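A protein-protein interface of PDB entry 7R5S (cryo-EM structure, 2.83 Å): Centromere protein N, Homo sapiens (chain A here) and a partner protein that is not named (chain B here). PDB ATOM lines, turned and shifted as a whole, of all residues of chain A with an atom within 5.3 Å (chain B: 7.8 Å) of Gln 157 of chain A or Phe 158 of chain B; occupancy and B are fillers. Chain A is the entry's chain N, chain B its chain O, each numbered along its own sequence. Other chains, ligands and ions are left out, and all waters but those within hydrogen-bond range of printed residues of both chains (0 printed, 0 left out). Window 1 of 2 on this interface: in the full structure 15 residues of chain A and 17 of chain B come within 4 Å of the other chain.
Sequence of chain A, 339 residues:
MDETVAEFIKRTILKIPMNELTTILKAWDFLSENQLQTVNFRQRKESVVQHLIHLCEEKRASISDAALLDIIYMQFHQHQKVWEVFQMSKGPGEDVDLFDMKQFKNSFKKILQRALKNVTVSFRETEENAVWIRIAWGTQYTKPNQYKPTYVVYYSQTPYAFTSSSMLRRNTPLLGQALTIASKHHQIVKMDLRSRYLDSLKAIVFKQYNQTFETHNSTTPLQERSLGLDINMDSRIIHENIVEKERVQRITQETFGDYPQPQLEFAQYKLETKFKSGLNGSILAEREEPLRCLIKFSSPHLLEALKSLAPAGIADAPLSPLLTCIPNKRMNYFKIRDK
The backbone NH (N) of Leu 214 of chain B sits at hydrogen-bond distance from the side-chain amide oxygen (OE1) of Gln 157 of chain A (2.8 Å).
The backbone NH (N) of Cys 215 of chain B lies within hydrogen-bond range of the side-chain amide oxygen (OD1) of Asn 212 of chain B (3.2 Å). The side-chain amide oxygen (OD1) of Asn 212 of chain B sits at hydrogen-bond distance from the backbone NH (N) of Asn 216 of chain B, 3.1 Å away.
Among the printed residues, pairs that only touch across the chains: Gln 157 of chain A with Pro 213 of chain B (3.4 Å), Leu 98 of chain A with Asn 216 of chain B (3.4 Å), Asn 129 of chain A with Pro 213 of chain B (3.5 Å), Gln 157 of chain A with Asn 216 of chain B (3.6 Å), Leu 98 of chain A with Leu 217 of chain B (3.7 Å), Phe 99 of chain A with Leu 217 of chain B (3.8 Å), Phe 99 of chain A with Asn 212 of chain B (3.8 Å), Ser 156 of chain A with Pro 213 of chain B (3.8 Å), Asp 97 of chain A with Asn 216 of chain B (3.8 Å), Gln 157 of chain A with Asn 212 of chain B (3.9 Å) and Gln 157 of chain A with Phe 158 of chain B (3.9 Å).
Of the printed residues of chain B, Asp 97 of chain A touches Asn 216 (3.8 Å). Printed residues of chain B within 4 Å of Asn 129 of chain A: Pro 213 (3.5 Å). Tyr 155 of chain A touches none of the printed residues of chain B. Gln 157 of chain A touches just these residues of chain B: Phe 158, Asn 212, Pro 213, Leu 214 and Asn 216. Phe 158 of chain B touches one residue of chain A. Of the printed residues of chain A, Leu 217 of chain B touches Leu 98 and Phe 99. The nearest residue of chain B that does not touch Gln 157 of chain A is Cys 215 of chain B (5.0 Å).
Among the printed residues, no Asp or Glu carboxylate lies within 4 Å of a Lys or Arg side-chain nitrogen of the other chain.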
ATOM      1  N   ASP A  97      25.989  -0.872  14.426  1.00  0.00           N
ATOM      2  CA  ASP A  97      25.384   0.031  15.391  1.00  0.00           C
ATOM      3  C   ASP A  97      24.763   1.237  14.695  1.00  0.00           C
ATOM      4  O   ASP A  97      25.134   1.605  13.578  1.00  0.00           O
ATOM      5  CB  ASP A  97      26.420   0.497  16.416  1.00  0.00           C
ATOM      6  CG  ASP A  97      27.496   1.370  15.801  1.00  0.00           C
ATOM      7  OD1 ASP A  97      27.853   1.139  14.627  1.00  0.00           O
ATOM      8  OD2 ASP A  97      27.984   2.290  16.491  1.00  0.00           O
ATOM      9  N   LEU A  98      23.803   1.852  15.379  1.00  0.00           N
ATOM     10  CA  LEU A  98      23.157   3.079  14.918  1.00  0.00           C
ATOM     11  C   LEU A  98      23.865   4.244  15.601  1.00  0.00           C
ATOM     12  O   LEU A  98      23.598   4.550  16.766  1.00  0.00           O
ATOM     13  CB  LEU A  98      21.664   3.063  15.227  1.00  0.00           C
ATOM     14  CG  LEU A  98      20.801   2.029  14.497  1.00  0.00           C
ATOM     15  CD1 LEU A  98      20.771   0.705  15.245  1.00  0.00           C
ATOM     16  CD2 LEU A  98      19.391   2.560  14.287  1.00  0.00           C
ATOM     17  N   PHE A  99      24.772   4.889  14.872  1.00  0.00           N
ATOM     18  CA  PHE A  99      25.607   5.929  15.455  1.00  0.00           C
ATOM     19  C   PHE A  99      24.773   7.143  15.845  1.00  0.00           C
ATOM     20  O   PHE A  99      23.928   7.606  15.072  1.00  0.00           O
ATOM     21  CB  PHE A  99      26.705   6.336  14.472  1.00  0.00           C
ATOM     22  CG  PHE A  99      27.639   7.384  15.006  1.00  0.00           C
ATOM     23  CD1 PHE A  99      28.652   7.043  15.884  1.00  0.00           C
ATOM     24  CD2 PHE A  99      27.506   8.708  14.624  1.00  0.00           C
ATOM     25  CE1 PHE A  99      29.512   8.004  16.377  1.00  0.00           C
ATOM     26  CE2 PHE A  99      28.364   9.672  15.113  1.00  0.00           C
ATOM     27  CZ  PHE A  99      29.368   9.320  15.990  1.00  0.00           C
ATOM     28  N   ASN A 129      31.745  13.884   7.325  1.00  0.00           N
ATOM     29  CA  ASN A 129      31.530  12.977   8.451  1.00  0.00           C
ATOM     30  C   ASN A 129      32.734  12.993   9.393  1.00  0.00           C
ATOM     31  O   ASN A 129      33.355  11.967   9.672  1.00  0.00           O
ATOM     32  CB  ASN A 129      31.220  11.559   7.962  1.00  0.00           C
ATOM     33  CG  ASN A 129      30.233  11.544   6.810  1.00  0.00           C
ATOM     34  OD1 ASN A 129      30.520  11.008   5.739  1.00  0.00           O
ATOM     35  ND2 ASN A 129      29.065  12.134   7.025  1.00  0.00           N
ATOM     36  N   TYR A 154      37.897  12.166  14.197  1.00  0.00           N
ATOM     37  CA  TYR A 154      37.201  10.889  14.146  1.00  0.00           C
ATOM     38  C   TYR A 154      36.183  10.885  13.014  1.00  0.00           C
ATOM     39  O   TYR A 154      35.458  11.865  12.811  1.00  0.00           O
ATOM     40  CB  TYR A 154      36.503  10.588  15.474  1.00  0.00           C
ATOM     41  CG  TYR A 154      35.705   9.304  15.459  1.00  0.00           C
ATOM     42  CD1 TYR A 154      36.334   8.075  15.316  1.00  0.00           C
ATOM     43  CD2 TYR A 154      34.323   9.322  15.588  1.00  0.00           C
ATOM     44  CE1 TYR A 154      35.609   6.899  15.301  1.00  0.00           C
ATOM     45  CE2 TYR A 154      33.591   8.151  15.573  1.00  0.00           C
ATOM     46  CZ  TYR A 154      34.238   6.943  15.430  1.00  0.00           C
ATOM     47  OH  TYR A 154      33.512   5.775  15.415  1.00  0.00           O
ATOM     48  N   TYR A 155      36.135   9.778  12.279  1.00  0.00           N
ATOM     49  CA  TYR A 155      35.182   9.582  11.195  1.00  0.00           C
ATOM     50  C   TYR A 155      34.137   8.573  11.647  1.00  0.00           C
ATOM     51  O   TYR A 155      34.478   7.444  12.015  1.00  0.00           O
ATOM     52  CB  TYR A 155      35.888   9.112   9.924  1.00  0.00           C
ATOM     53  CG  TYR A 155      36.555  10.232   9.165  1.00  0.00           C
ATOM     54  CD1 TYR A 155      37.795  10.719   9.555  1.00  0.00           C
ATOM     55  CD2 TYR A 155      35.943  10.809   8.063  1.00  0.00           C
ATOM     56  CE1 TYR A 155      38.405  11.747   8.866  1.00  0.00           C
ATOM     57  CE2 TYR A 155      36.545  11.836   7.368  1.00  0.00           C
ATOM     58  CZ  TYR A 155      37.775  12.301   7.774  1.00  0.00           C
ATOM     59  OH  TYR A 155      38.377  13.326   7.085  1.00  0.00           O
ATOM     60  N   SER A 156      32.871   8.982  11.619  1.00  0.00           N
ATOM     61  CA  SER A 156      31.801   8.168  12.177  1.00  0.00           C
ATOM     62  C   SER A 156      31.622   6.876  11.390  1.00  0.00           C
ATOM     63  O   SER A 156      31.777   6.845  10.167  1.00  0.00           O
ATOM     64  CB  SER A 156      30.493   8.957  12.191  1.00  0.00           C
ATOM     65  OG  SER A 156      30.701  10.278  12.657  1.00  0.00           O
ATOM     66  N   GLN A 157      31.293   5.803  12.113  1.00  0.00           N
ATOM     67  CA  GLN A 157      31.012   4.485  11.545  1.00  0.00           C
ATOM     68  C   GLN A 157      32.189   3.918  10.756  1.00  0.00           C
ATOM     69  O   GLN A 157      31.999   3.075   9.875  1.00  0.00           O
ATOM     70  CB  GLN A 157      29.751   4.518  10.675  1.00  0.00           C
ATOM     71  CG  GLN A 157      28.481   4.809  11.461  1.00  0.00           C
ATOM     72  CD  GLN A 157      27.267   4.977  10.573  1.00  0.00           C
ATOM     73  OE1 GLN A 157      27.307   5.701   9.579  1.00  0.00           O
ATOM     74  NE2 GLN A 157      26.177   4.309  10.929  1.00  0.00           N
ATOM     75  N   THR A 158      33.406   4.366  11.057  1.00  0.00           N
ATOM     76  CA  THR A 158      34.621   3.834  10.465  1.00  0.00           C
ATOM     77  C   THR A 158      35.596   3.425  11.564  1.00  0.00           C
ATOM     78  O   THR A 158      35.593   4.012  12.650  1.00  0.00           O
ATOM     79  CB  THR A 158      35.300   4.858   9.545  1.00  0.00           C
ATOM     80  OG1 THR A 158      35.694   6.000  10.311  1.00  0.00           O
ATOM     81  CG2 THR A 158      34.353   5.294   8.436  1.00  0.00           C
ATOM     82  N   PRO A 159      36.440   2.422  11.316  1.00  0.00           N
ATOM     83  CA  PRO A 159      37.387   1.965  12.338  1.00  0.00           C
ATOM     84  C   PRO A 159      38.646   2.809  12.467  1.00  0.00           C
ATOM     85  O   PRO A 159      39.579   2.380  13.150  1.00  0.00           O
ATOM     86  CB  PRO A 159      37.745   0.543  11.864  1.00  0.00           C
ATOM     87  CG  PRO A 159      36.780   0.218  10.754  1.00  0.00           C
ATOM     88  CD  PRO A 159      36.424   1.526  10.150  1.00  0.00           C
ATOM     89  N   TYR B 138      29.341   3.604  -8.999  1.00  0.00           N
ATOM     90  CA  TYR B 138      30.545   3.135  -8.328  1.00  0.00           C
ATOM     91  C   TYR B 138      31.236   2.085  -9.188  1.00  0.00           C
ATOM     92  O   TYR B 138      30.631   1.492 -10.084  1.00  0.00           O
ATOM     93  CB  TYR B 138      30.224   2.566  -6.939  1.00  0.00           C
ATOM     94  CG  TYR B 138      29.423   3.513  -6.074  1.00  0.00           C
ATOM     95  CD1 TYR B 138      30.051   4.499  -5.324  1.00  0.00           C
ATOM     96  CD2 TYR B 138      28.038   3.427  -6.014  1.00  0.00           C
ATOM     97  CE1 TYR B 138      29.324   5.368  -4.536  1.00  0.00           C
ATOM     98  CE2 TYR B 138      27.303   4.293  -5.228  1.00  0.00           C
ATOM     99  CZ  TYR B 138      27.951   5.262  -4.491  1.00  0.00           C
ATOM    100  OH  TYR B 138      27.223   6.126  -3.707  1.00  0.00           O
ATOM    101  N   VAL B 155      33.865   2.189  -3.528  1.00  0.00           N
ATOM    102  CA  VAL B 155      32.778   1.995  -2.561  1.00  0.00           C
ATOM    103  C   VAL B 155      33.098   2.772  -1.289  1.00  0.00           C
ATOM    104  O   VAL B 155      34.262   2.779  -0.852  1.00  0.00           O
ATOM    105  CB  VAL B 155      32.593   0.504  -2.267  1.00  0.00           C
ATOM    106  CG1 VAL B 155      31.436   0.277  -1.307  1.00  0.00           C
ATOM    107  CG2 VAL B 155      32.373  -0.264  -3.561  1.00  0.00           C
ATOM    108  N   PRO B 156      32.126   3.451  -0.677  1.00  0.00           N
ATOM    109  CA  PRO B 156      32.399   4.172   0.572  1.00  0.00           C
ATOM    110  C   PRO B 156      32.908   3.245   1.668  1.00  0.00           C
ATOM    111  O   PRO B 156      32.747   2.024   1.620  1.00  0.00           O
ATOM    112  CB  PRO B 156      31.038   4.773   0.939  1.00  0.00           C
ATOM    113  CG  PRO B 156      30.332   4.909  -0.364  1.00  0.00           C
ATOM    114  CD  PRO B 156      30.778   3.742  -1.197  1.00  0.00           C
ATOM    115  N   VAL B 157      33.530   3.856   2.677  1.00  0.00           N
ATOM    116  CA  VAL B 157      34.197   3.081   3.718  1.00  0.00           C
ATOM    117  C   VAL B 157      33.181   2.451   4.663  1.00  0.00           C
ATOM    118  O   VAL B 157      33.345   1.305   5.097  1.00  0.00           O
ATOM    119  CB  VAL B 157      35.203   3.965   4.477  1.00  0.00           C
ATOM    120  CG1 VAL B 157      36.035   3.126   5.432  1.00  0.00           C
ATOM    121  CG2 VAL B 157      36.094   4.714   3.497  1.00  0.00           C
ATOM    122  N   PHE B 158      32.117   3.183   4.998  1.00  0.00           N
ATOM    123  CA  PHE B 158      31.135   2.673   5.948  1.00  0.00           C
ATOM    124  C   PHE B 158      30.281   1.547   5.379  1.00  0.00           C
ATOM    125  O   PHE B 158      29.558   0.899   6.143  1.00  0.00           O
ATOM    126  CB  PHE B 158      30.232   3.808   6.439  1.00  0.00           C
ATOM    127  CG  PHE B 158      29.938   4.849   5.398  1.00  0.00           C
ATOM    128  CD1 PHE B 158      28.926   4.655   4.473  1.00  0.00           C
ATOM    129  CD2 PHE B 158      30.666   6.025   5.350  1.00  0.00           C
ATOM    130  CE1 PHE B 158      28.651   5.613   3.517  1.00  0.00           C
ATOM    131  CE2 PHE B 158      30.396   6.985   4.396  1.00  0.00           C
ATOM    132  CZ  PHE B 158      29.387   6.780   3.479  1.00  0.00           C
ATOM    133  N   ILE B 159      30.345   1.297   4.079  1.00  0.00           N
ATOM    134  CA  ILE B 159      29.597   0.189   3.482  1.00  0.00           C
ATOM    135  C   ILE B 159      30.324  -1.116   3.792  1.00  0.00           C
ATOM    136  O   ILE B 159      31.529  -1.222   3.521  1.00  0.00           O
ATOM    137  CB  ILE B 159      29.445   0.390   1.979  1.00  0.00           C
ATOM    138  CG1 ILE B 159      28.590   1.626   1.690  1.00  0.00           C
ATOM    139  CG2 ILE B 159      28.826  -0.842   1.336  1.00  0.00           C
ATOM    140  CD1 ILE B 159      27.174   1.520   2.203  1.00  0.00           C
ATOM    141  N   PRO B 160      29.643  -2.118   4.353  1.00  0.00           N
ATOM    142  CA  PRO B 160      30.327  -3.375   4.691  1.00  0.00           C
ATOM    143  C   PRO B 160      30.672  -4.201   3.463  1.00  0.00           C
ATOM    144  O   PRO B 160      29.975  -5.167   3.137  1.00  0.00           O
ATOM    145  CB  PRO B 160      29.309  -4.094   5.585  1.00  0.00           C
ATOM    146  CG  PRO B 160      27.988  -3.561   5.145  1.00  0.00           C
ATOM    147  CD  PRO B 160      28.226  -2.128   4.755  1.00  0.00           C
ATOM    148  N   LEU B 161      31.753  -3.829   2.776  1.00  0.00           N
ATOM    149  CA  LEU B 161      32.175  -4.562   1.588  1.00  0.00           C
ATOM    150  C   LEU B 161      33.052  -5.758   1.932  1.00  0.00           C
ATOM    151  O   LEU B 161      32.996  -6.782   1.240  1.00  0.00           O
ATOM    152  CB  LEU B 161      32.916  -3.625   0.631  1.00  0.00           C
ATOM    153  CG  LEU B 161      33.559  -4.249  -0.609  1.00  0.00           C
ATOM    154  CD1 LEU B 161      32.505  -4.879  -1.505  1.00  0.00           C
ATOM    155  CD2 LEU B 161      34.370  -3.216  -1.374  1.00  0.00           C
ATOM    156  N   TYR B 183      22.799  -3.282  -1.667  1.00  0.00           N
ATOM    157  CA  TYR B 183      23.295  -2.407  -0.607  1.00  0.00           C
ATOM    158  C   TYR B 183      23.442  -0.972  -1.101  1.00  0.00           C
ATOM    159  O   TYR B 183      22.984  -0.024  -0.446  1.00  0.00           O
ATOM    160  CB  TYR B 183      24.628  -2.933  -0.076  1.00  0.00           C
ATOM    161  CG  TYR B 183      24.499  -3.909   1.072  1.00  0.00           C
ATOM    162  CD1 TYR B 183      24.137  -5.230   0.848  1.00  0.00           C
ATOM    163  CD2 TYR B 183      24.746  -3.511   2.378  1.00  0.00           C
ATOM    164  CE1 TYR B 183      24.021  -6.126   1.892  1.00  0.00           C
ATOM    165  CE2 TYR B 183      24.632  -4.400   3.430  1.00  0.00           C
ATOM    166  CZ  TYR B 183      24.269  -5.706   3.180  1.00  0.00           C
ATOM    167  OH  TYR B 183      24.154  -6.595   4.223  1.00  0.00           O
ATOM    168  N   TYR B 187      21.296   2.352   0.153  1.00  0.00           N
ATOM    169  CA  TYR B 187      21.979   3.515   0.715  1.00  0.00           C
ATOM    170  C   TYR B 187      21.662   4.778  -0.079  1.00  0.00           C
ATOM    171  O   TYR B 187      21.375   5.833   0.506  1.00  0.00           O
ATOM    172  CB  TYR B 187      23.486   3.267   0.757  1.00  0.00           C
ATOM    173  CG  TYR B 187      24.313   4.526   0.885  1.00  0.00           C
ATOM    174  CD1 TYR B 187      24.333   5.247   2.070  1.00  0.00           C
ATOM    175  CD2 TYR B 187      25.078   4.988  -0.177  1.00  0.00           C
ATOM    176  CE1 TYR B 187      25.089   6.397   2.192  1.00  0.00           C
ATOM    177  CE2 TYR B 187      25.837   6.136  -0.063  1.00  0.00           C
ATOM    178  CZ  TYR B 187      25.838   6.836   1.123  1.00  0.00           C
ATOM    179  OH  TYR B 187      26.592   7.980   1.241  1.00  0.00           O
ATOM    180  N   LYS B 191      19.693   8.098   1.394  1.00  0.00           N
ATOM    181  CA  LYS B 191      20.343   9.404   1.367  1.00  0.00           C
ATOM    182  C   LYS B 191      19.543  10.401   0.536  1.00  0.00           C
ATOM    183  O   LYS B 191      19.437  11.578   0.902  1.00  0.00           O
ATOM    184  CB  LYS B 191      21.767   9.276   0.828  1.00  0.00           C
ATOM    185  CG  LYS B 191      22.604  10.530   1.004  1.00  0.00           C
ATOM    186  CD  LYS B 191      24.056  10.287   0.631  1.00  0.00           C
ATOM    187  CE  LYS B 191      24.201   9.990  -0.851  1.00  0.00           C
ATOM    188  NZ  LYS B 191      23.772  11.142  -1.690  1.00  0.00           N
ATOM    189  N   ARG B 211      21.546  13.154  11.543  1.00  0.00           N
ATOM    190  CA  ARG B 211      21.761  12.128  10.535  1.00  0.00           C
ATOM    191  C   ARG B 211      23.181  11.592  10.656  1.00  0.00           C
ATOM    192  O   ARG B 211      24.112  12.329  10.990  1.00  0.00           O
ATOM    193  CB  ARG B 211      21.508  12.680   9.127  1.00  0.00           C
ATOM    194  CG  ARG B 211      21.528  11.637   8.024  1.00  0.00           C
ATOM    195  CD  ARG B 211      21.163  12.255   6.685  1.00  0.00           C
ATOM    196  NE  ARG B 211      22.030  13.380   6.349  1.00  0.00           N
ATOM    197  CZ  ARG B 211      21.912  14.111   5.246  1.00  0.00           C
ATOM    198  NH1 ARG B 211      20.961  13.836   4.365  1.00  0.00           N
ATOM    199  NH2 ARG B 211      22.745  15.117   5.022  1.00  0.00           N
ATOM    200  N   ASN B 212      23.331  10.302  10.382  1.00  0.00           N
ATOM    201  CA  ASN B 212      24.611   9.614  10.392  1.00  0.00           C
ATOM    202  C   ASN B 212      25.074   9.331   8.968  1.00  0.00           C
ATOM    203  O   ASN B 212      24.279   9.400   8.024  1.00  0.00           O
ATOM    204  CB  ASN B 212      24.507   8.301  11.183  1.00  0.00           C
ATOM    205  CG  ASN B 212      23.234   7.542  10.886  1.00  0.00           C
ATOM    206  OD1 ASN B 212      22.459   7.925  10.012  1.00  0.00           O
ATOM    207  ND2 ASN B 212      23.009   6.455  11.614  1.00  0.00           N
ATOM    208  N   PRO B 213      26.364   9.032   8.768  1.00  0.00           N
ATOM    209  CA  PRO B 213      26.845   8.779   7.396  1.00  0.00           C
ATOM    210  C   PRO B 213      26.106   7.662   6.680  1.00  0.00           C
ATOM    211  O   PRO B 213      25.813   7.790   5.484  1.00  0.00           O
ATOM    212  CB  PRO B 213      28.325   8.433   7.610  1.00  0.00           C
ATOM    213  CG  PRO B 213      28.692   9.131   8.863  1.00  0.00           C
ATOM    214  CD  PRO B 213      27.475   9.092   9.737  1.00  0.00           C
ATOM    215  N   LEU B 214      25.794   6.567   7.373  1.00  0.00           N
ATOM    216  CA  LEU B 214      25.094   5.456   6.740  1.00  0.00           C
ATOM    217  C   LEU B 214      23.615   5.745   6.514  1.00  0.00           C
ATOM    218  O   LEU B 214      22.966   4.998   5.774  1.00  0.00           O
ATOM    219  CB  LEU B 214      25.256   4.190   7.584  1.00  0.00           C
ATOM    220  CG  LEU B 214      25.086   2.845   6.876  1.00  0.00           C
ATOM    221  CD1 LEU B 214      26.042   2.734   5.703  1.00  0.00           C
ATOM    222  CD2 LEU B 214      25.299   1.701   7.852  1.00  0.00           C
ATOM    223  N   CYS B 215      23.076   6.802   7.126  1.00  0.00           N
ATOM    224  CA  CYS B 215      21.673   7.191   6.974  1.00  0.00           C
ATOM    225  C   CYS B 215      20.735   6.059   7.394  1.00  0.00           C
ATOM    226  O   CYS B 215      19.851   5.640   6.646  1.00  0.00           O
ATOM    227  CB  CYS B 215      21.378   7.647   5.541  1.00  0.00           C
ATOM    228  SG  CYS B 215      22.271   9.133   5.032  1.00  0.00           S
ATOM    229  N   ASN B 216      20.934   5.566   8.618  1.00  0.00           N
ATOM    230  CA  ASN B 216      20.101   4.511   9.182  1.00  0.00           C
ATOM    231  C   ASN B 216      19.489   4.923  10.517  1.00  0.00           C
ATOM    232  O   ASN B 216      18.991   4.069  11.259  1.00  0.00           O
ATOM    233  CB  ASN B 216      20.904   3.219   9.340  1.00  0.00           C
ATOM    234  CG  ASN B 216      22.132   3.398  10.206  1.00  0.00           C
ATOM    235  OD1 ASN B 216      22.676   4.496  10.312  1.00  0.00           O
ATOM    236  ND2 ASN B 216      22.578   2.316  10.832  1.00  0.00           N
ATOM    237  N   LEU B 217      19.515   6.216  10.836  1.00  0.00           N
ATOM    238  CA  LEU B 217      18.933   6.714  12.080  1.00  0.00           C
ATOM    239  C   LEU B 217      18.579   8.179  11.866  1.00  0.00           C
ATOM    240  O   LEU B 217      19.477   9.015  11.728  1.00  0.00           O
ATOM    241  CB  LEU B 217      19.906   6.540  13.244  1.00  0.00           C
ATOM    242  CG  LEU B 217      19.540   7.166  14.592  1.00  0.00           C
ATOM    243  CD1 LEU B 217      19.846   6.205  15.725  1.00  0.00           C
ATOM    244  CD2 LEU B 217      20.284   8.476  14.803  1.00  0.00           C
ATOM    245  N   LEU B 242      19.638  -3.002   6.400  1.00  0.00           N
ATOM    246  CA  LEU B 242      20.429  -2.188   5.484  1.00  0.00           C
ATOM    247  C   LEU B 242      20.120  -2.462   4.017  1.00  0.00           C
ATOM    248  O   LEU B 242      20.789  -1.895   3.146  1.00  0.00           O
ATOM    249  CB  LEU B 242      21.922  -2.405   5.746  1.00  0.00           C
ATOM    250  CG  LEU B 242      22.634  -1.338   6.582  1.00  0.00           C
ATOM    251  CD1 LEU B 242      21.931  -1.127   7.911  1.00  0.00           C
ATOM    252  CD2 LEU B 242      24.090  -1.719   6.800  1.00  0.00           C
